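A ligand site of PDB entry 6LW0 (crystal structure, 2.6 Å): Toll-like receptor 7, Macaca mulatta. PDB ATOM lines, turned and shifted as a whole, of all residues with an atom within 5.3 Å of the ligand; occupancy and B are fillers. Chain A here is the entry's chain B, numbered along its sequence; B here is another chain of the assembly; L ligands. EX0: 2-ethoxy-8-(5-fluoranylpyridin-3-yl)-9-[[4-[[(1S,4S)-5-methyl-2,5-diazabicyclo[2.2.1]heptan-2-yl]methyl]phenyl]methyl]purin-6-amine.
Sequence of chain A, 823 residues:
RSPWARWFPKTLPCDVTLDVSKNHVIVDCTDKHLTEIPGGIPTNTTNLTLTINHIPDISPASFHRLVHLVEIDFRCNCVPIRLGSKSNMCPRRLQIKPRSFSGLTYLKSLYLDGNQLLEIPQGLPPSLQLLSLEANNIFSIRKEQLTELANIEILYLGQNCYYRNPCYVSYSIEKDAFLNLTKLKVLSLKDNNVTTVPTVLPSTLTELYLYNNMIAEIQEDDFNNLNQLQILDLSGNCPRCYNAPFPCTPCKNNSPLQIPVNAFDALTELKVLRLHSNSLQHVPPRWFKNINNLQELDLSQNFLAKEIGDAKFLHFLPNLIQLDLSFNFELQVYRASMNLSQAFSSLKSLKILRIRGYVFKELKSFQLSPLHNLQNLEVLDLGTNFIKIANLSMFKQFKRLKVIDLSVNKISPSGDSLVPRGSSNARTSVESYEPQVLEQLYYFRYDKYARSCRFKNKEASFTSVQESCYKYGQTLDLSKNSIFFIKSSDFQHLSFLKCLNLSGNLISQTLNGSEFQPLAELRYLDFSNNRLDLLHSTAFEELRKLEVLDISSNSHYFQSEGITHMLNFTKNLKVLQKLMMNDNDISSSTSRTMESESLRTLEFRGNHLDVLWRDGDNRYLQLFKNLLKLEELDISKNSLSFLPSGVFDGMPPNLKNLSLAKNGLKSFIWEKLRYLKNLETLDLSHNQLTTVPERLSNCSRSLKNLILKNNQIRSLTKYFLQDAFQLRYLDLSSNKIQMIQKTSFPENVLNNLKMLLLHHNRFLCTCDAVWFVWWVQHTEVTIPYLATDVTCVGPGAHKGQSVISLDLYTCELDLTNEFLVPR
A nitrogen (N4) of the ligand lies within hydrogen-bond range of the side-chain carboxylate of Asp 533.
A nitrogen (N1) of the ligand is in hydrogen-bond range of the backbone NH of Thr 564, at 3.0 Å.
N4 of the ligand lies within hydrogen-bond range of O of Thr 564, 3.1 Å away.
OH of Tyr 334 of chain B is in hydrogen-bond range of N5 of the ligand, at 3.1 Å.
The side-chain carboxylate of Asp 533 is in salt-bridge range of the side-chain amino group of Lys 410 of chain B, at 3.5 Å.
OD1 of Asp 533 sits close to N of Leu 535.
The side-chain hydroxyl of Tyr 242 of chain B is in hydrogen-bond range of the side-chain amide nitrogen of Gln 332 of chain B, 3.3 Å away.
OH of Tyr 242 of chain B is in hydrogen-bond range of OG1 of Thr 564.
OG1 of Thr 564 is in hydrogen-bond range of ND2 of Asn 243 of chain B, at 2.8 Å.
The side-chain hydroxyl (OH) of Tyr 334 of chain B is in hydrogen-bond range of the backbone carbonyl oxygen (O) of Phe 386 of chain B (2.5 Å).
The side-chain amino group (NZ) of Lys 410 of chain B lies within hydrogen-bond range of the backbone carbonyl oxygen (O) of Ser 508 (2.5 Å).
A fluorine (F) of the ligand lies close to the backbone NH of Thr 510 (3.4 Å).
The side-chain amino group (NZ) of Lys 410 of chain B sits close to a fluorine (F) of the ligand (3.3 Å).
CA of Gln 509 touches F of the ligand (3.7 Å).
CD2 of Leu 535 touches C10 of the ligand (3.7 Å).
O of Gly 562 touches C6 of the ligand, 3.6 Å away.
Ile 563 touches the ligand (CG2 to N4, 3.3 Å).
O of Gln 332 of chain B touches C20 of the ligand, 2.9 Å away.
CG1 of Val 359 of chain B touches C12 of the ligand, at 3.9 Å.
Phe 386 of chain B touches the ligand.
Lys 388 of chain B touches the ligand.
Hydrophobic or aromatic side chains that line the ligand: Leu 535, Ile 563, Tyr 334 of chain B, Val 359 of chain B and Phe 386 of chain B.
Within 4 Å of the ligand: Gln 509, Thr 510, Asp 533, Leu 535, Gly 562, Ile 563, Thr 564, Gln 332 of chain B, Tyr 334 of chain B, Val 359 of chain B, Phe 386 of chain B, Lys 388 of chain B and Lys 410 of chain B.
Along chain A the residues within 4 Å of the ligand span positions 509 to 564.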
ATOM      1  N   SER A 508     -12.395  13.342 -16.963  1.00  0.00           N
ATOM      2  CA  SER A 508     -11.842  12.056 -17.365  1.00  0.00           C
ATOM      3  C   SER A 508     -10.627  12.256 -18.248  1.00  0.00           C
ATOM      4  O   SER A 508     -10.374  11.496 -19.188  1.00  0.00           O
ATOM      5  CB  SER A 508     -12.906  11.212 -18.076  1.00  0.00           C
ATOM      6  OG  SER A 508     -13.690  12.007 -18.939  1.00  0.00           O
ATOM      7  N   GLN A 509      -9.783  13.219 -17.892  1.00  0.00           N
ATOM      8  CA  GLN A 509      -8.709  13.695 -18.751  1.00  0.00           C
ATOM      9  C   GLN A 509      -7.378  13.427 -18.066  1.00  0.00           C
ATOM     10  O   GLN A 509      -7.317  13.167 -16.865  1.00  0.00           O
ATOM     11  CB  GLN A 509      -8.859  15.194 -19.083  1.00  0.00           C
ATOM     12  CG  GLN A 509      -8.379  16.182 -18.014  1.00  0.00           C
ATOM     13  CD  GLN A 509      -8.743  17.633 -18.333  1.00  0.00           C
ATOM     14  OE1 GLN A 509      -9.867  18.072 -18.107  1.00  0.00           O
ATOM     15  NE2 GLN A 509      -7.784  18.385 -18.857  1.00  0.00           N
ATOM     16  N   THR A 510      -6.339  13.369 -18.877  1.00  0.00           N
ATOM     17  CA  THR A 510      -4.982  13.146 -18.368  1.00  0.00           C
ATOM     18  C   THR A 510      -4.406  14.477 -17.913  1.00  0.00           C
ATOM     19  O   THR A 510      -3.761  15.195 -18.679  1.00  0.00           O
ATOM     20  CB  THR A 510      -4.112  12.509 -19.454  1.00  0.00           C
ATOM     21  OG1 THR A 510      -4.353  13.141 -20.711  1.00  0.00           O
ATOM     22  CG2 THR A 510      -4.469  11.075 -19.589  1.00  0.00           C
ATOM     23  N   ASP A 533      -7.257  10.318 -14.784  1.00  0.00           N
ATOM     24  CA  ASP A 533      -6.381   9.498 -15.613  1.00  0.00           C
ATOM     25  C   ASP A 533      -4.936   9.872 -15.309  1.00  0.00           C
ATOM     26  O   ASP A 533      -4.442  10.882 -15.817  1.00  0.00           O
ATOM     27  CB  ASP A 533      -6.723   9.689 -17.068  1.00  0.00           C
ATOM     28  CG  ASP A 533      -6.019   8.696 -17.946  1.00  0.00           C
ATOM     29  OD1 ASP A 533      -5.156   7.942 -17.463  1.00  0.00           O
ATOM     30  OD2 ASP A 533      -6.355   8.661 -19.140  1.00  0.00           O
ATOM     31  N   LEU A 534      -4.254   9.055 -14.481  1.00  0.00           N
ATOM     32  CA  LEU A 534      -2.867   9.303 -14.057  1.00  0.00           C
ATOM     33  C   LEU A 534      -1.844   8.800 -15.052  1.00  0.00           C
ATOM     34  O   LEU A 534      -0.844   8.184 -14.681  1.00  0.00           O
ATOM     35  CB  LEU A 534      -2.614   8.669 -12.696  1.00  0.00           C
ATOM     36  CG  LEU A 534      -3.146   9.473 -11.507  1.00  0.00           C
ATOM     37  CD1 LEU A 534      -2.961   8.688 -10.206  1.00  0.00           C
ATOM     38  CD2 LEU A 534      -2.468  10.848 -11.428  1.00  0.00           C
ATOM     39  N   LEU A 535      -2.070   9.103 -16.337  1.00  0.00           N
ATOM     40  CA  LEU A 535      -1.052   8.861 -17.348  1.00  0.00           C
ATOM     41  C   LEU A 535       0.240   9.621 -17.062  1.00  0.00           C
ATOM     42  O   LEU A 535       1.345   9.107 -17.282  1.00  0.00           O
ATOM     43  CB  LEU A 535      -1.603   9.240 -18.709  1.00  0.00           C
ATOM     44  CG  LEU A 535      -0.552   9.208 -19.806  1.00  0.00           C
ATOM     45  CD1 LEU A 535      -0.100   7.783 -19.973  1.00  0.00           C
ATOM     46  CD2 LEU A 535      -1.110   9.790 -21.097  1.00  0.00           C
ATOM     47  N   HIS A 536       0.145  10.862 -16.581  1.00  0.00           N
ATOM     48  CA  HIS A 536       1.307  11.707 -16.341  1.00  0.00           C
ATOM     49  C   HIS A 536       1.572  11.873 -14.862  1.00  0.00           C
ATOM     50  O   HIS A 536       0.672  12.286 -14.105  1.00  0.00           O
ATOM     51  CB  HIS A 536       1.126  13.091 -16.975  1.00  0.00           C
ATOM     52  CG  HIS A 536       0.778  13.051 -18.424  1.00  0.00           C
ATOM     53  ND1 HIS A 536       1.565  12.424 -19.354  1.00  0.00           N
ATOM     54  CD2 HIS A 536      -0.274  13.563 -19.100  1.00  0.00           C
ATOM     55  CE1 HIS A 536       1.005  12.544 -20.546  1.00  0.00           C
ATOM     56  NE2 HIS A 536      -0.107  13.234 -20.414  1.00  0.00           N
ATOM     57  N   GLY A 562      -4.095  -2.723 -18.600  1.00  0.00           N
ATOM     58  CA  GLY A 562      -3.245  -2.170 -19.634  1.00  0.00           C
ATOM     59  C   GLY A 562      -3.180  -0.666 -19.636  1.00  0.00           C
ATOM     60  O   GLY A 562      -2.548  -0.090 -20.539  1.00  0.00           O
ATOM     61  N   ILE A 563      -3.882  -0.014 -18.745  1.00  0.00           N
ATOM     62  CA  ILE A 563      -3.820   1.425 -18.621  1.00  0.00           C
ATOM     63  C   ILE A 563      -2.653   1.799 -17.708  1.00  0.00           C
ATOM     64  O   ILE A 563      -2.381   1.126 -16.711  1.00  0.00           O
ATOM     65  CB  ILE A 563      -5.175   1.935 -18.115  1.00  0.00           C
ATOM     66  CG1 ILE A 563      -6.184   1.781 -19.250  1.00  0.00           C
ATOM     67  CG2 ILE A 563      -5.086   3.382 -17.657  1.00  0.00           C
ATOM     68  CD1 ILE A 563      -7.586   1.664 -18.797  1.00  0.00           C
ATOM     69  N   THR A 564      -1.953   2.873 -18.058  1.00  0.00           N
ATOM     70  CA  THR A 564      -0.844   3.368 -17.246  1.00  0.00           C
ATOM     71  C   THR A 564      -1.352   4.261 -16.109  1.00  0.00           C
ATOM     72  O   THR A 564      -2.149   5.174 -16.334  1.00  0.00           O
ATOM     73  CB  THR A 564       0.158   4.126 -18.117  1.00  0.00           C
ATOM     74  OG1 THR A 564       0.945   3.181 -18.835  1.00  0.00           O
ATOM     75  CG2 THR A 564       1.081   4.964 -17.279  1.00  0.00           C
ATOM     76  N   TYR B 242       5.799  -4.366 -20.657  1.00  0.00           N
ATOM     77  CA  TYR B 242       5.277  -3.064 -20.264  1.00  0.00           C
ATOM     78  C   TYR B 242       3.989  -3.206 -19.458  1.00  0.00           C
ATOM     79  O   TYR B 242       3.051  -3.867 -19.905  1.00  0.00           O
ATOM     80  CB  TYR B 242       5.018  -2.191 -21.501  1.00  0.00           C
ATOM     81  CG  TYR B 242       4.700  -0.751 -21.151  1.00  0.00           C
ATOM     82  CD1 TYR B 242       5.613   0.031 -20.442  1.00  0.00           C
ATOM     83  CD2 TYR B 242       3.480  -0.168 -21.515  1.00  0.00           C
ATOM     84  CE1 TYR B 242       5.340   1.352 -20.113  1.00  0.00           C
ATOM     85  CE2 TYR B 242       3.177   1.175 -21.188  1.00  0.00           C
ATOM     86  CZ  TYR B 242       4.116   1.922 -20.476  1.00  0.00           C
ATOM     87  OH  TYR B 242       3.852   3.242 -20.142  1.00  0.00           O
ATOM     88  N   ASN B 243       3.944  -2.569 -18.290  1.00  0.00           N
ATOM     89  CA  ASN B 243       2.792  -2.660 -17.394  1.00  0.00           C
ATOM     90  C   ASN B 243       2.405  -4.118 -17.126  1.00  0.00           C
ATOM     91  O   ASN B 243       1.229  -4.477 -17.049  1.00  0.00           O
ATOM     92  CB  ASN B 243       1.607  -1.853 -17.925  1.00  0.00           C
ATOM     93  CG  ASN B 243       1.765  -0.355 -17.700  1.00  0.00           C
ATOM     94  OD1 ASN B 243       2.368   0.073 -16.713  1.00  0.00           O
ATOM     95  ND2 ASN B 243       1.200   0.446 -18.600  1.00  0.00           N
ATOM     96  N   PHE B 329       0.973  -1.540 -29.752  1.00  0.00           N
ATOM     97  CA  PHE B 329       1.386  -0.153 -29.863  1.00  0.00           C
ATOM     98  C   PHE B 329       2.845  -0.027 -29.491  1.00  0.00           C
ATOM     99  O   PHE B 329       3.340  -0.704 -28.585  1.00  0.00           O
ATOM    100  CB  PHE B 329       0.530   0.728 -28.941  1.00  0.00           C
ATOM    101  CG  PHE B 329       0.784   0.491 -27.471  1.00  0.00           C
ATOM    102  CD1 PHE B 329       0.176  -0.582 -26.823  1.00  0.00           C
ATOM    103  CD2 PHE B 329       1.641   1.306 -26.754  1.00  0.00           C
ATOM    104  CE1 PHE B 329       0.431  -0.818 -25.481  1.00  0.00           C
ATOM    105  CE2 PHE B 329       1.894   1.077 -25.406  1.00  0.00           C
ATOM    106  CZ  PHE B 329       1.287   0.019 -24.775  1.00  0.00           C
ATOM    107  N   GLN B 332       4.859   4.817 -25.890  1.00  0.00           N
ATOM    108  CA  GLN B 332       4.842   6.280 -25.866  1.00  0.00           C
ATOM    109  C   GLN B 332       4.462   6.919 -27.206  1.00  0.00           C
ATOM    110  O   GLN B 332       4.823   8.079 -27.456  1.00  0.00           O
ATOM    111  CB  GLN B 332       6.162   6.875 -25.355  1.00  0.00           C
ATOM    112  CG  GLN B 332       6.627   6.370 -23.993  1.00  0.00           C
ATOM    113  CD  GLN B 332       5.504   6.266 -22.944  1.00  0.00           C
ATOM    114  OE1 GLN B 332       4.552   7.066 -22.932  1.00  0.00           O
ATOM    115  NE2 GLN B 332       5.645   5.302 -22.032  1.00  0.00           N
ATOM    116  N   VAL B 333       3.767   6.215 -28.090  1.00  0.00           N
ATOM    117  CA  VAL B 333       3.257   6.809 -29.317  1.00  0.00           C
ATOM    118  C   VAL B 333       1.728   6.835 -29.252  1.00  0.00           C
ATOM    119  O   VAL B 333       1.099   5.875 -28.796  1.00  0.00           O
ATOM    120  CB  VAL B 333       3.779   6.086 -30.561  1.00  0.00           C
ATOM    121  CG1 VAL B 333       3.269   6.767 -31.797  1.00  0.00           C
ATOM    122  CG2 VAL B 333       5.266   6.192 -30.542  1.00  0.00           C
ATOM    123  N   TYR B 334       1.146   7.956 -29.682  1.00  0.00           N
ATOM    124  CA  TYR B 334      -0.303   8.095 -29.781  1.00  0.00           C
ATOM    125  C   TYR B 334      -0.680   8.365 -31.247  1.00  0.00           C
ATOM    126  O   TYR B 334      -0.955   9.501 -31.637  1.00  0.00           O
ATOM    127  CB  TYR B 334      -0.778   9.242 -28.816  1.00  0.00           C
ATOM    128  CG  TYR B 334      -2.268   9.252 -28.511  1.00  0.00           C
ATOM    129  CD1 TYR B 334      -3.112   8.268 -29.002  1.00  0.00           C
ATOM    130  CD2 TYR B 334      -2.811  10.283 -27.762  1.00  0.00           C
ATOM    131  CE1 TYR B 334      -4.468   8.293 -28.725  1.00  0.00           C
ATOM    132  CE2 TYR B 334      -4.160  10.315 -27.474  1.00  0.00           C
ATOM    133  CZ  TYR B 334      -4.985   9.319 -27.961  1.00  0.00           C
ATOM    134  OH  TYR B 334      -6.330   9.385 -27.667  1.00  0.00           O
ATOM    135  N   VAL B 359      -3.839   2.063 -30.006  1.00  0.00           N
ATOM    136  CA  VAL B 359      -3.687   3.389 -29.413  1.00  0.00           C
ATOM    137  C   VAL B 359      -3.590   4.497 -30.447  1.00  0.00           C
ATOM    138  O   VAL B 359      -2.484   4.958 -30.781  1.00  0.00           O
ATOM    139  CB  VAL B 359      -2.482   3.415 -28.450  1.00  0.00           C
ATOM    140  CG1 VAL B 359      -2.509   4.676 -27.622  1.00  0.00           C
ATOM    141  CG2 VAL B 359      -2.506   2.197 -27.549  1.00  0.00           C
ATOM    142  N   THR B 384      -9.977  -0.558 -25.867  1.00  0.00           N
ATOM    143  CA  THR B 384      -8.770  -0.055 -25.228  1.00  0.00           C
ATOM    144  C   THR B 384      -7.811   0.503 -26.269  1.00  0.00           C
ATOM    145  O   THR B 384      -6.689   0.042 -26.437  1.00  0.00           O
ATOM    146  CB  THR B 384      -8.099  -1.116 -24.347  1.00  0.00           C
ATOM    147  OG1 THR B 384      -9.074  -1.656 -23.461  1.00  0.00           O
ATOM    148  CG2 THR B 384      -7.021  -0.492 -23.492  1.00  0.00           C
ATOM    149  N   PHE B 386      -8.166   4.185 -26.885  1.00  0.00           N
ATOM    150  CA  PHE B 386      -8.134   5.609 -26.606  1.00  0.00           C
ATOM    151  C   PHE B 386      -8.527   6.417 -27.835  1.00  0.00           C
ATOM    152  O   PHE B 386      -7.990   7.496 -28.079  1.00  0.00           O
ATOM    153  CB  PHE B 386      -6.763   6.012 -26.071  1.00  0.00           C
ATOM    154  CG  PHE B 386      -6.442   5.386 -24.748  1.00  0.00           C
ATOM    155  CD1 PHE B 386      -6.867   5.979 -23.559  1.00  0.00           C
ATOM    156  CD2 PHE B 386      -5.766   4.173 -24.691  1.00  0.00           C
ATOM    157  CE1 PHE B 386      -6.591   5.384 -22.351  1.00  0.00           C
ATOM    158  CE2 PHE B 386      -5.489   3.578 -23.484  1.00  0.00           C
ATOM    159  CZ  PHE B 386      -5.900   4.191 -22.314  1.00  0.00           C
ATOM    160  N   LYS B 388     -10.583   8.964 -29.699  1.00  0.00           N
ATOM    161  CA  LYS B 388     -11.341  10.142 -29.305  1.00  0.00           C
ATOM    162  C   LYS B 388     -12.459  10.510 -30.274  1.00  0.00           C
ATOM    163  O   LYS B 388     -13.407  11.200 -29.870  1.00  0.00           O
ATOM    164  CB  LYS B 388     -10.399  11.352 -29.157  1.00  0.00           C
ATOM    165  CG  LYS B 388      -9.436  11.306 -27.952  1.00  0.00           C
ATOM    166  CD  LYS B 388      -8.329  12.344 -28.108  1.00  0.00           C
ATOM    167  CE  LYS B 388      -8.020  13.065 -26.811  1.00  0.00           C
ATOM    168  NZ  LYS B 388      -7.293  14.335 -27.072  1.00  0.00           N
ATOM    169  N   LYS B 410     -12.230   6.753 -25.626  1.00  0.00           N
ATOM    170  CA  LYS B 410     -12.501   8.132 -25.238  1.00  0.00           C
ATOM    171  C   LYS B 410     -13.420   8.819 -26.233  1.00  0.00           C
ATOM    172  O   LYS B 410     -13.268  10.009 -26.516  1.00  0.00           O
ATOM    173  CB  LYS B 410     -11.195   8.912 -25.115  1.00  0.00           C
ATOM    174  CG  LYS B 410     -10.296   8.409 -24.031  1.00  0.00           C
ATOM    175  CD  LYS B 410     -10.309   9.357 -22.864  1.00  0.00           C
ATOM    176  CE  LYS B 410      -9.233   8.991 -21.862  1.00  0.00           C
ATOM    177  NZ  LYS B 410      -9.283   9.859 -20.658  1.00  0.00           N
HETATM  178  N   EX0 L   1      -2.551   5.305 -22.546  1.00  0.00           N
HETATM  179  C   EX0 L   1      -3.859   6.800 -21.096  1.00  0.00           C
HETATM  180  O   EX0 L   1      -1.395   3.426 -21.552  1.00  0.00           O
HETATM  181  C1  EX0 L   1      -3.350   6.406 -22.422  1.00  0.00           C
HETATM  182  C10 EX0 L   1      -0.710   9.734 -24.728  1.00  0.00           C
HETATM  183  C11 EX0 L   1       0.401   8.914 -24.846  1.00  0.00           C
HETATM  184  C12 EX0 L   1      -1.024   6.982 -24.880  1.00  0.00           C
HETATM  185  C13 EX0 L   1       0.249   7.530 -24.935  1.00  0.00           C
HETATM  186  C14 EX0 L   1      -5.400   9.434 -23.123  1.00  0.00           C
HETATM  187  C15 EX0 L   1      -6.065  10.310 -22.253  1.00  0.00           C
HETATM  188  C16 EX0 L   1      -5.577   9.684 -24.474  1.00  0.00           C
HETATM  189  C17 EX0 L   1      -6.830  11.405 -22.721  1.00  0.00           C
HETATM  190  C18 EX0 L   1      -6.922  11.571 -24.090  1.00  0.00           C
HETATM  191  C19 EX0 L   1       1.780   9.527 -24.900  1.00  0.00           C
HETATM  192  C2  EX0 L   1      -3.452   5.946 -19.951  1.00  0.00           C
HETATM  193  C20 EX0 L   1       3.392  10.417 -26.428  1.00  0.00           C
HETATM  194  C21 EX0 L   1       1.635  11.871 -25.716  1.00  0.00           C
HETATM  195  C22 EX0 L   1       3.325  11.877 -26.334  1.00  0.00           C
HETATM  196  C23 EX0 L   1       1.677  12.688 -27.037  1.00  0.00           C
HETATM  197  C24 EX0 L   1       3.316  11.991 -28.674  1.00  0.00           C
HETATM  198  C25 EX0 L   1       2.890  12.357 -25.025  1.00  0.00           C
HETATM  199  C3  EX0 L   1      -2.223   4.541 -21.454  1.00  0.00           C
HETATM  200  C4  EX0 L   1      -4.606   8.247 -22.597  1.00  0.00           C
HETATM  201  C5  EX0 L   1      -1.196   2.678 -22.747  1.00  0.00           C
HETATM  202  C6  EX0 L   1      -2.538   2.196 -23.259  1.00  0.00           C
HETATM  203  C7  EX0 L   1      -3.531   7.243 -24.699  1.00  0.00           C
HETATM  204  C8  EX0 L   1      -2.134   7.816 -24.779  1.00  0.00           C
HETATM  205  C9  EX0 L   1      -1.977   9.184 -24.686  1.00  0.00           C
HETATM  206  F   EX0 L   1      -7.466  12.289 -21.901  1.00  0.00           F
HETATM  207  N1  EX0 L   1      -2.659   4.869 -20.201  1.00  0.00           N
HETATM  208  N2  EX0 L   1      -4.605   7.912 -21.274  1.00  0.00           N
HETATM  209  N3  EX0 L   1      -3.861   7.310 -23.274  1.00  0.00           N
HETATM  210  N4  EX0 L   1      -3.886   6.245 -18.711  1.00  0.00           N
HETATM  211  N5  EX0 L   1      -6.306  10.720 -24.924  1.00  0.00           N
HETATM  212  N6  EX0 L   1       1.954  10.431 -26.048  1.00  0.00           N
HETATM  213  N7  EX0 L   1       3.110  12.734 -27.426  1.00  0.00           N
